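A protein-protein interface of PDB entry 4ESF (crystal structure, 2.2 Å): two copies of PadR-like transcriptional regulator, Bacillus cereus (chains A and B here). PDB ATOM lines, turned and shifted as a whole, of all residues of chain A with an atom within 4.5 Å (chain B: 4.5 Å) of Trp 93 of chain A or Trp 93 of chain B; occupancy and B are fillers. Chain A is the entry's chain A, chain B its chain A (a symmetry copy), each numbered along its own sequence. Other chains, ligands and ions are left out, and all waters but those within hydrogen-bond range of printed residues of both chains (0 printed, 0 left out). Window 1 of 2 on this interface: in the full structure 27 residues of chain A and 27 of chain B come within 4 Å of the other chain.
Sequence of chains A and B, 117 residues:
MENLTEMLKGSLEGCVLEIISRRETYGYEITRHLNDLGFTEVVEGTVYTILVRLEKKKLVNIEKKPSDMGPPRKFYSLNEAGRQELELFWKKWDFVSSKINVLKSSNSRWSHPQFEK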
ATOM      1  N   MET A   7      16.785   9.368  11.564  1.00  0.00           N
ATOM      2  CA  MET A   7      17.867   9.747  12.468  1.00  0.00           C
ATOM      3  C   MET A   7      17.392   9.809  13.913  1.00  0.00           C
ATOM      4  O   MET A   7      18.106   9.412  14.838  1.00  0.00           O
ATOM      5  CB  MET A   7      18.443  11.101  12.056  1.00  0.00           C
ATOM      6  CG  MET A   7      19.609  11.572  12.913  1.00  0.00           C
ATOM      7  SD  MET A   7      20.343  13.092  12.264  1.00  0.00           S
ATOM      8  CE  MET A   7      21.188  12.521  10.776  1.00  0.00           C
ATOM      9  N   SER A  11      16.645   7.299  18.865  1.00  0.00           N
ATOM     10  CA  SER A  11      16.847   8.092  20.094  1.00  0.00           C
ATOM     11  C   SER A  11      15.551   8.542  20.753  1.00  0.00           C
ATOM     12  O   SER A  11      15.550   9.118  21.839  1.00  0.00           O
ATOM     13  CB  SER A  11      17.650   9.349  19.786  1.00  0.00           C
ATOM     14  OG  SER A  11      18.998   9.034  19.488  1.00  0.00           O
ATOM     15  N   PHE A  89      20.555   4.991  28.477  1.00  0.00           N
ATOM     16  CA  PHE A  89      20.309   5.686  27.214  1.00  0.00           C
ATOM     17  C   PHE A  89      21.235   6.886  27.072  1.00  0.00           C
ATOM     18  O   PHE A  89      21.825   7.088  26.028  1.00  0.00           O
ATOM     19  CB  PHE A  89      18.852   6.167  27.141  1.00  0.00           C
ATOM     20  CG  PHE A  89      18.630   7.237  26.119  1.00  0.00           C
ATOM     21  CD1 PHE A  89      18.603   6.922  24.750  1.00  0.00           C
ATOM     22  CD2 PHE A  89      18.430   8.548  26.512  1.00  0.00           C
ATOM     23  CE1 PHE A  89      18.389   7.911  23.785  1.00  0.00           C
ATOM     24  CE2 PHE A  89      18.205   9.557  25.559  1.00  0.00           C
ATOM     25  CZ  PHE A  89      18.179   9.243  24.194  1.00  0.00           C
ATOM     26  N   TRP A  90      21.338   7.692  28.124  1.00  0.00           N
ATOM     27  CA  TRP A  90      22.164   8.888  28.077  1.00  0.00           C
ATOM     28  C   TRP A  90      23.651   8.506  27.957  1.00  0.00           C
ATOM     29  O   TRP A  90      24.407   9.197  27.278  1.00  0.00           O
ATOM     30  CB  TRP A  90      21.922   9.797  29.298  1.00  0.00           C
ATOM     31  CG  TRP A  90      20.632  10.628  29.204  1.00  0.00           C
ATOM     32  CD1 TRP A  90      19.600  10.672  30.117  1.00  0.00           C
ATOM     33  CD2 TRP A  90      20.257  11.505  28.130  1.00  0.00           C
ATOM     34  NE1 TRP A  90      18.603  11.526  29.659  1.00  0.00           N
ATOM     35  CE2 TRP A  90      18.985  12.044  28.446  1.00  0.00           C
ATOM     36  CE3 TRP A  90      20.868  11.879  26.927  1.00  0.00           C
ATOM     37  CZ2 TRP A  90      18.326  12.957  27.604  1.00  0.00           C
ATOM     38  CZ3 TRP A  90      20.204  12.773  26.082  1.00  0.00           C
ATOM     39  CH2 TRP A  90      18.947  13.301  26.426  1.00  0.00           C
ATOM     40  N   LYS A  91      24.082   7.416  28.602  1.00  0.00           N
ATOM     41  CA  LYS A  91      25.486   6.995  28.470  1.00  0.00           C
ATOM     42  C   LYS A  91      25.735   6.601  27.002  1.00  0.00           C
ATOM     43  O   LYS A  91      26.677   7.070  26.373  1.00  0.00           O
ATOM     44  CB  LYS A  91      25.835   5.857  29.439  1.00  0.00           C
ATOM     45  CG  LYS A  91      27.318   5.486  29.405  1.00  0.00           C
ATOM     46  CD  LYS A  91      27.722   4.424  30.446  1.00  0.00           C
ATOM     47  CE  LYS A  91      27.150   3.051  30.133  1.00  0.00           C
ATOM     48  NZ  LYS A  91      27.594   2.535  28.803  1.00  0.00           N
ATOM     49  N   LYS A  92      24.849   5.785  26.443  1.00  0.00           N
ATOM     50  CA  LYS A  92      24.902   5.478  25.028  1.00  0.00           C
ATOM     51  C   LYS A  92      24.880   6.747  24.144  1.00  0.00           C
ATOM     52  O   LYS A  92      25.728   6.915  23.258  1.00  0.00           O
ATOM     53  CB  LYS A  92      23.773   4.516  24.658  1.00  0.00           C
ATOM     54  CG  LYS A  92      24.000   3.130  25.254  1.00  0.00           C
ATOM     55  CD  LYS A  92      22.956   2.096  24.842  1.00  0.00           C
ATOM     56  CE  LYS A  92      21.561   2.487  25.320  1.00  0.00           C
ATOM     57  NZ  LYS A  92      20.549   1.404  25.130  1.00  0.00           N
ATOM     58  N   TRP A  93      23.953   7.665  24.406  1.00  0.00           N
ATOM     59  CA  TRP A  93      23.897   8.903  23.633  1.00  0.00           C
ATOM     60  C   TRP A  93      25.238   9.655  23.669  1.00  0.00           C
ATOM     61  O   TRP A  93      25.758  10.065  22.629  1.00  0.00           O
ATOM     62  CB  TRP A  93      22.788   9.832  24.168  1.00  0.00           C
ATOM     63  CG  TRP A  93      22.931  11.204  23.592  1.00  0.00           C
ATOM     64  CD1 TRP A  93      23.331  12.335  24.234  1.00  0.00           C
ATOM     65  CD2 TRP A  93      22.733  11.553  22.229  1.00  0.00           C
ATOM     66  NE1 TRP A  93      23.376  13.384  23.345  1.00  0.00           N
ATOM     67  CE2 TRP A  93      23.022  12.925  22.103  1.00  0.00           C
ATOM     68  CE3 TRP A  93      22.340  10.837  21.092  1.00  0.00           C
ATOM     69  CZ2 TRP A  93      22.913  13.598  20.897  1.00  0.00           C
ATOM     70  CZ3 TRP A  93      22.248  11.502  19.895  1.00  0.00           C
ATOM     71  CH2 TRP A  93      22.518  12.881  19.810  1.00  0.00           C
ATOM     72  N   ASP A  94      25.784   9.843  24.870  1.00  0.00           N
ATOM     73  CA  ASP A  94      27.036  10.599  25.042  1.00  0.00           C
ATOM     74  C   ASP A  94      28.187   9.984  24.247  1.00  0.00           C
ATOM     75  O   ASP A  94      28.988  10.682  23.636  1.00  0.00           O
ATOM     76  CB  ASP A  94      27.437  10.672  26.506  1.00  0.00           C
ATOM     77  CG  ASP A  94      26.556  11.604  27.305  1.00  0.00           C
ATOM     78  OD1 ASP A  94      25.956  12.537  26.717  1.00  0.00           O
ATOM     79  OD2 ASP A  94      26.465  11.408  28.537  1.00  0.00           O
ATOM     80  N   PHE A  95      28.261   8.667  24.271  1.00  0.00           N
ATOM     81  CA  PHE A  95      29.289   7.957  23.537  1.00  0.00           C
ATOM     82  C   PHE A  95      29.118   8.128  22.033  1.00  0.00           C
ATOM     83  O   PHE A  95      30.040   8.556  21.329  1.00  0.00           O
ATOM     84  CB  PHE A  95      29.258   6.463  23.883  1.00  0.00           C
ATOM     85  CG  PHE A  95      30.299   5.657  23.149  1.00  0.00           C
ATOM     86  CD1 PHE A  95      31.620   5.660  23.573  1.00  0.00           C
ATOM     87  CD2 PHE A  95      29.961   4.918  22.022  1.00  0.00           C
ATOM     88  CE1 PHE A  95      32.574   4.938  22.894  1.00  0.00           C
ATOM     89  CE2 PHE A  95      30.923   4.181  21.347  1.00  0.00           C
ATOM     90  CZ  PHE A  95      32.223   4.198  21.778  1.00  0.00           C
ATOM     91  N   VAL A  96      27.936   7.776  21.541  1.00  0.00           N
ATOM     92  CA  VAL A  96      27.666   7.818  20.112  1.00  0.00           C
ATOM     93  C   VAL A  96      27.830   9.236  19.549  1.00  0.00           C
ATOM     94  O   VAL A  96      28.489   9.425  18.521  1.00  0.00           O
ATOM     95  CB  VAL A  96      26.253   7.304  19.814  1.00  0.00           C
ATOM     96  CG1 VAL A  96      25.817   7.663  18.384  1.00  0.00           C
ATOM     97  CG2 VAL A  96      26.209   5.810  20.019  1.00  0.00           C
ATOM     98  N   SER A  97      27.236  10.230  20.216  1.00  0.00           N
ATOM     99  CA  SER A  97      27.309  11.611  19.736  1.00  0.00           C
ATOM    100  C   SER A  97      28.732  12.200  19.785  1.00  0.00           C
ATOM    101  O   SER A  97      29.176  12.828  18.835  1.00  0.00           O
ATOM    102  CB  SER A  97      26.323  12.498  20.502  1.00  0.00           C
ATOM    103  OG  SER A  97      26.652  12.628  21.879  1.00  0.00           O
ATOM    104  N   ILE A 100      30.580  10.692  16.743  1.00  0.00           N
ATOM    105  CA  ILE A 100      30.126  11.320  15.515  1.00  0.00           C
ATOM    106  C   ILE A 100      30.636  12.768  15.394  1.00  0.00           C
ATOM    107  O   ILE A 100      31.074  13.177  14.321  1.00  0.00           O
ATOM    108  CB  ILE A 100      28.617  11.255  15.430  1.00  0.00           C
ATOM    109  CG1 ILE A 100      28.224   9.806  15.131  1.00  0.00           C
ATOM    110  CG2 ILE A 100      28.095  12.259  14.384  1.00  0.00           C
ATOM    111  CD1 ILE A 100      26.747   9.534  15.219  1.00  0.00           C
ATOM    112  N   ASN A 101      30.605  13.529  16.482  1.00  0.00           N
ATOM    113  CA  ASN A 101      31.210  14.854  16.471  1.00  0.00           C
ATOM    114  C   ASN A 101      32.735  14.867  16.272  1.00  0.00           C
ATOM    115  O   ASN A 101      33.276  15.836  15.720  1.00  0.00           O
ATOM    116  CB  ASN A 101      30.848  15.624  17.736  1.00  0.00           C
ATOM    117  CG  ASN A 101      29.390  16.050  17.748  1.00  0.00           C
ATOM    118  OD1 ASN A 101      28.767  16.202  16.693  1.00  0.00           O
ATOM    119  ND2 ASN A 101      28.838  16.239  18.940  1.00  0.00           N
ATOM    120  N   LYS A 104      32.865  14.632  12.574  1.00  0.00           N
ATOM    121  CA  LYS A 104      32.472  15.893  11.978  1.00  0.00           C
ATOM    122  C   LYS A 104      33.613  16.892  12.097  1.00  0.00           C
ATOM    123  O   LYS A 104      33.855  17.679  11.183  1.00  0.00           O
ATOM    124  CB  LYS A 104      31.240  16.453  12.700  1.00  0.00           C
ATOM    125  CG  LYS A 104      30.684  17.742  12.113  1.00  0.00           C
ATOM    126  CD  LYS A 104      29.513  18.249  12.937  1.00  0.00           C
ATOM    127  CE  LYS A 104      29.981  19.042  14.146  1.00  0.00           C
ATOM    128  NZ  LYS A 104      28.918  19.195  15.190  1.00  0.00           N
ATOM    129  N   MET B   7      20.703   2.976  17.832  1.00  0.00           N
ATOM    130  CA  MET B   7      20.967   4.408  17.934  1.00  0.00           C
ATOM    131  C   MET B   7      21.851   4.896  16.794  1.00  0.00           C
ATOM    132  O   MET B   7      21.654   5.988  16.255  1.00  0.00           O
ATOM    133  CB  MET B   7      21.632   4.724  19.273  1.00  0.00           C
ATOM    134  CG  MET B   7      21.915   6.203  19.499  1.00  0.00           C
ATOM    135  SD  MET B   7      22.543   6.516  21.165  1.00  0.00           S
ATOM    136  CE  MET B   7      21.084   6.260  22.194  1.00  0.00           C
ATOM    137  N   SER B  11      22.345   7.066  11.653  1.00  0.00           N
ATOM    138  CA  SER B  11      23.441   8.020  11.394  1.00  0.00           C
ATOM    139  C   SER B  11      24.620   7.411  10.647  1.00  0.00           C
ATOM    140  O   SER B  11      25.561   8.102  10.264  1.00  0.00           O
ATOM    141  CB  SER B  11      23.983   8.572  12.707  1.00  0.00           C
ATOM    142  OG  SER B  11      23.051   9.448  13.316  1.00  0.00           O
ATOM    143  N   PHE B  89      23.176  15.752   5.583  1.00  0.00           N
ATOM    144  CA  PHE B  89      23.271  14.854   6.733  1.00  0.00           C
ATOM    145  C   PHE B  89      23.790  15.600   7.954  1.00  0.00           C
ATOM    146  O   PHE B  89      23.250  15.463   9.034  1.00  0.00           O
ATOM    147  CB  PHE B  89      24.214  13.682   6.422  1.00  0.00           C
ATOM    148  CG  PHE B  89      24.706  12.976   7.646  1.00  0.00           C
ATOM    149  CD1 PHE B  89      23.858  12.114   8.362  1.00  0.00           C
ATOM    150  CD2 PHE B  89      26.009  13.148   8.077  1.00  0.00           C
ATOM    151  CE1 PHE B  89      24.307  11.441   9.502  1.00  0.00           C
ATOM    152  CE2 PHE B  89      26.484  12.476   9.216  1.00  0.00           C
ATOM    153  CZ  PHE B  89      25.639  11.618   9.930  1.00  0.00           C
ATOM    154  N   TRP B  90      24.859  16.370   7.778  1.00  0.00           N
ATOM    155  CA  TRP B  90      25.458  17.091   8.889  1.00  0.00           C
ATOM    156  C   TRP B  90      24.496  18.180   9.401  1.00  0.00           C
ATOM    157  O   TRP B  90      24.440  18.430  10.602  1.00  0.00           O
ATOM    158  CB  TRP B  90      26.824  17.695   8.507  1.00  0.00           C
ATOM    159  CG  TRP B  90      27.970  16.670   8.494  1.00  0.00           C
ATOM    160  CD1 TRP B  90      28.830  16.394   7.452  1.00  0.00           C
ATOM    161  CD2 TRP B  90      28.347  15.795   9.570  1.00  0.00           C
ATOM    162  NE1 TRP B  90      29.714  15.388   7.826  1.00  0.00           N
ATOM    163  CE2 TRP B  90      29.435  15.008   9.115  1.00  0.00           C
ATOM    164  CE3 TRP B  90      27.864  15.594  10.868  1.00  0.00           C
ATOM    165  CZ2 TRP B  90      30.059  14.048   9.931  1.00  0.00           C
ATOM    166  CZ3 TRP B  90      28.473  14.626  11.672  1.00  0.00           C
ATOM    167  CH2 TRP B  90      29.559  13.866  11.199  1.00  0.00           C
ATOM    168  N   LYS B  91      23.736  18.826   8.510  1.00  0.00           N
ATOM    169  CA  LYS B  91      22.771  19.839   8.970  1.00  0.00           C
ATOM    170  C   LYS B  91      21.704  19.131   9.827  1.00  0.00           C
ATOM    171  O   LYS B  91      21.417  19.545  10.945  1.00  0.00           O
ATOM    172  CB  LYS B  91      22.150  20.610   7.798  1.00  0.00           C
ATOM    173  CG  LYS B  91      21.236  21.747   8.257  1.00  0.00           C
ATOM    174  CD  LYS B  91      20.685  22.612   7.106  1.00  0.00           C
ATOM    175  CE  LYS B  91      19.681  21.864   6.242  1.00  0.00           C
ATOM    176  NZ  LYS B  91      18.499  21.387   7.021  1.00  0.00           N
ATOM    177  N   LYS B  92      21.164  18.029   9.321  1.00  0.00           N
ATOM    178  CA  LYS B  92      20.269  17.204  10.107  1.00  0.00           C
ATOM    179  C   LYS B  92      20.900  16.754  11.446  1.00  0.00           C
ATOM    180  O   LYS B  92      20.297  16.915  12.515  1.00  0.00           O
ATOM    181  CB  LYS B  92      19.795  16.009   9.280  1.00  0.00           C
ATOM    182  CG  LYS B  92      18.860  16.442   8.155  1.00  0.00           C
ATOM    183  CD  LYS B  92      18.276  15.285   7.351  1.00  0.00           C
ATOM    184  CE  LYS B  92      19.366  14.485   6.645  1.00  0.00           C
ATOM    185  NZ  LYS B  92      18.828  13.482   5.678  1.00  0.00           N
ATOM    186  N   TRP B  93      22.126  16.239  11.408  1.00  0.00           N
ATOM    187  CA  TRP B  93      22.795  15.825  12.638  1.00  0.00           C
ATOM    188  C   TRP B  93      22.868  16.974  13.657  1.00  0.00           C
ATOM    189  O   TRP B  93      22.522  16.799  14.828  1.00  0.00           O
ATOM    190  CB  TRP B  93      24.225  15.328  12.344  1.00  0.00           C
ATOM    191  CG  TRP B  93      25.008  15.201  13.610  1.00  0.00           C
ATOM    192  CD1 TRP B  93      26.034  15.989  14.034  1.00  0.00           C
ATOM    193  CD2 TRP B  93      24.763  14.256  14.643  1.00  0.00           C
ATOM    194  NE1 TRP B  93      26.459  15.573  15.274  1.00  0.00           N
ATOM    195  CE2 TRP B  93      25.686  14.515  15.673  1.00  0.00           C
ATOM    196  CE3 TRP B  93      23.846  13.210  14.801  1.00  0.00           C
ATOM    197  CZ2 TRP B  93      25.732  13.758  16.834  1.00  0.00           C
ATOM    198  CZ3 TRP B  93      23.884  12.472  15.958  1.00  0.00           C
ATOM    199  CH2 TRP B  93      24.838  12.740  16.957  1.00  0.00           C
ATOM    200  N   ASP B  94      23.329  18.142  13.209  1.00  0.00           N
ATOM    201  CA  ASP B  94      23.501  19.301  14.100  1.00  0.00           C
ATOM    202  C   ASP B  94      22.189  19.700  14.776  1.00  0.00           C
ATOM    203  O   ASP B  94      22.150  20.028  15.956  1.00  0.00           O
ATOM    204  CB  ASP B  94      24.045  20.501  13.342  1.00  0.00           C
ATOM    205  CG  ASP B  94      25.502  20.343  12.974  1.00  0.00           C
ATOM    206  OD1 ASP B  94      26.230  19.582  13.658  1.00  0.00           O
ATOM    207  OD2 ASP B  94      25.928  20.991  11.992  1.00  0.00           O
ATOM    208  N   PHE B  95      21.117  19.675  14.006  1.00  0.00           N
ATOM    209  CA  PHE B  95      19.807  20.005  14.530  1.00  0.00           C
ATOM    210  C   PHE B  95      19.346  18.983  15.562  1.00  0.00           C
ATOM    211  O   PHE B  95      19.001  19.332  16.696  1.00  0.00           O
ATOM    212  CB  PHE B  95      18.779  20.074  13.393  1.00  0.00           C
ATOM    213  CG  PHE B  95      17.387  20.408  13.865  1.00  0.00           C
ATOM    214  CD1 PHE B  95      17.041  21.717  14.168  1.00  0.00           C
ATOM    215  CD2 PHE B  95      16.434  19.410  14.028  1.00  0.00           C
ATOM    216  CE1 PHE B  95      15.776  22.020  14.615  1.00  0.00           C
ATOM    217  CE2 PHE B  95      15.155  19.720  14.466  1.00  0.00           C
ATOM    218  CZ  PHE B  95      14.832  21.018  14.764  1.00  0.00           C
ATOM    219  N   VAL B  96      19.327  17.719  15.157  1.00  0.00           N
ATOM    220  CA  VAL B  96      18.836  16.654  16.017  1.00  0.00           C
ATOM    221  C   VAL B  96      19.653  16.556  17.313  1.00  0.00           C
ATOM    222  O   VAL B  96      19.080  16.483  18.405  1.00  0.00           O
ATOM    223  CB  VAL B  96      18.867  15.309  15.283  1.00  0.00           C
ATOM    224  CG1 VAL B  96      18.697  14.134  16.261  1.00  0.00           C
ATOM    225  CG2 VAL B  96      17.782  15.284  14.235  1.00  0.00           C
ATOM    226  N   SER B  97      20.984  16.554  17.197  1.00  0.00           N
ATOM    227  CA  SER B  97      21.844  16.429  18.374  1.00  0.00           C
ATOM    228  C   SER B  97      21.759  17.639  19.324  1.00  0.00           C
ATOM    229  O   SER B  97      21.660  17.474  20.530  1.00  0.00           O
ATOM    230  CB  SER B  97      23.294  16.164  17.953  1.00  0.00           C
ATOM    231  OG  SER B  97      23.875  17.259  17.256  1.00  0.00           O
ATOM    232  N   ILE B 100      18.455  17.187  21.278  1.00  0.00           N
ATOM    233  CA  ILE B 100      18.597  16.139  22.272  1.00  0.00           C
ATOM    234  C   ILE B 100      19.492  16.582  23.443  1.00  0.00           C
ATOM    235  O   ILE B 100      19.165  16.323  24.599  1.00  0.00           O
ATOM    236  CB  ILE B 100      19.119  14.878  21.621  1.00  0.00           C
ATOM    237  CG1 ILE B 100      17.989  14.277  20.781  1.00  0.00           C
ATOM    238  CG2 ILE B 100      19.669  13.912  22.688  1.00  0.00           C
ATOM    239  CD1 ILE B 100      18.410  13.129  19.906  1.00  0.00           C
ATOM    240  N   ASN B 101      20.596  17.264  23.156  1.00  0.00           N
ATOM    241  CA  ASN B 101      21.403  17.840  24.222  1.00  0.00           C
ATOM    242  C   ASN B 101      20.706  18.941  25.040  1.00  0.00           C
ATOM    243  O   ASN B 101      21.016  19.116  26.227  1.00  0.00           O
ATOM    244  CB  ASN B 101      22.726  18.363  23.675  1.00  0.00           C
ATOM    245  CG  ASN B 101      23.665  17.237  23.275  1.00  0.00           C
ATOM    246  OD1 ASN B 101      23.570  16.122  23.795  1.00  0.00           O
ATOM    247  ND2 ASN B 101      24.568  17.522  22.346  1.00  0.00           N
ATOM    248  N   LYS B 104      18.825  16.820  27.430  1.00  0.00           N
ATOM    249  CA  LYS B 104      19.728  16.245  28.406  1.00  0.00           C
ATOM    250  C   LYS B 104      20.116  17.303  29.429  1.00  0.00           C
ATOM    251  O   LYS B 104      20.241  17.010  30.617  1.00  0.00           O
ATOM    252  CB  LYS B 104      20.996  15.734  27.711  1.00  0.00           C
ATOM    253  CG  LYS B 104      21.992  15.036  28.626  1.00  0.00           C
ATOM    254  CD  LYS B 104      23.237  14.630  27.858  1.00  0.00           C
ATOM    255  CE  LYS B 104      24.217  15.784  27.731  1.00  0.00           C
ATOM    256  NZ  LYS B 104      25.234  15.570  26.652  1.00  0.00           N
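Of the printed residues of chain B, Phe 89 of chain A touches Met 7. Trp 93 of chain A touches just these residues of chain B: Met 7 (3.7 Å), Trp 93 (3.7 Å), Ser 97 (3.9 Å), Ile 100 (3.5 Å) and Asn 101 (2.8 Å). Printed residues of chain B within 4 Å of Val 96 of chain A: Met 7 (3.9 Å). Printed residues of chain B within 4 Å of Ile 100 of chain A: Ser 11 (3.9 Å), Trp 90 (3.5 Å) and Trp 93 (3.5 Å). Lys 91 of chain B touches none of the printed residues of chain A. Trp 93 of chain B touches five residues of chain A. Phe 95 of chain B touches none of the printed residues of chain A. Printed residues of chain A within 4 Å of Asn 101 of chain B: Trp 93 (2.8 Å). The nearest residue of chain A that does not touch Trp 93 of chain B is Lys 104 of chain A (4.3 Å).
Phe 89 of chain B touches Met 7 of chain A (CE1 to CE, 3.5 Å). Met 7 of chain A touches Val 96 of chain B (SD to CG2, 3.9 Å). Phe 89 of chain A touches Met 7 of chain B. Trp 90 of chain A touches Ile 100 of chain B (CH2 to O, 3.5 Å). CH2 of Trp 90 of chain A touches CB of Lys 104 of chain B, at 3.4 Å. C of Lys 92 of chain A touches SD of Met 7 of chain B, 3.8 Å away. Trp 93 of chain A touches Ser 97 of chain B (CH2 to CB, 3.9 Å). CD1 of Ile 100 of chain A touches CB of Ser 11 of chain B, 3.9 Å away. Ile 100 of chain A touches Trp 93 of chain B. Trp 90 of chain B touches Lys 104 of chain A (CH2 to CB, 3.4 Å).
Of the 14 printed residues of chain B, 12 touch a printed residue of chain A. Hydrophobic or aromatic side chains of chain B that line the printed part of chain A: Met 7, Phe 89, Trp 90, Trp 93, Val 96 and Ile 100. Among the printed residues, Asp or Glu carboxylates within 4 Å of a Lys or Arg side-chain nitrogen of the other chain: Asp 94 of chain A with Lys 104 of chain B (3.1 Å) and Lys 104 of chain A with Asp 94 of chain B (3.1 Å).
OD1 of Asn 101 of chain B is in hydrogen-bond range of NZ of Lys 104 of chain B (3.4 Å). OG of Ser 97 of chain A lies within hydrogen-bond range of O of Trp 93 of chain A, at 2.8 Å. O of Trp 93 of chain B lies within hydrogen-bond range of OG of Ser 97 of chain B, 2.8 Å away. The side-chain amide oxygen (OD1) of Asn 101 of chain A lies within hydrogen-bond range of the side-chain amino group (NZ) of Lys 104 of chain A, at 3.4 Å. O of Ser 97 of chain B sits close to ND2 of Asn 101 of chain B (3.4 Å). The side-chain amide nitrogen (ND2) of Asn 101 of chain A lies close to the backbone carbonyl oxygen (O) of Ser 97 of chain A (3.4 Å).
The indole nitrogen (NE1) of Trp 93 of chain B sits at hydrogen-bond distance from the side-chain amide oxygen (OD1) of Asn 101 of chain A, 2.8 Å away. SD of Met 7 of chain A sits close to N of Trp 93 of chain B (3.7 Å). The side-chain carboxylate (OD1) of Asp 94 of chain A lies within salt-bridge range of the side-chain amino group (NZ) of Lys 104 of chain B (3.1 Å). The side-chain amide oxygen (OD1) of Asn 101 of chain B lies within hydrogen-bond range of the indole nitrogen (NE1) of Trp 93 of chain A (2.8 Å). The side-chain amino group (NZ) of Lys 104 of chain A is in salt-bridge range of the side-chain carboxylate (OD1) of Asp 94 of chain B (3.1 Å). The backbone NH of Trp 93 of chain A sits close to the side-chain sulfur of Met 7 of chain B, at 3.7 Å.
Met 7 of chain A touches Trp 93 of chain B, and with the chains exchanged Trp 93 of chain A touches Met 7 of chain B. Met 7 of chain A touches Val 96 of chain B, and with the chains exchanged Val 96 of chain A touches Met 7 of chain B. Trp 93 of chain B touches its own counterpart, Trp 93 of chain A. Asp 94 of chain A touches Lys 104 of chain B, and with the chains exchanged Lys 104 of chain A touches Asp 94 of chain B. Positions printed for both chains: 7, 11, 89, 90, 91, 92, 93, 94, 95, 96, 97, 100, 101 and 104. Of the 23 pairs that touch across the chains among the printed residues, 23 have their exchanged pair printed and touching as well.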
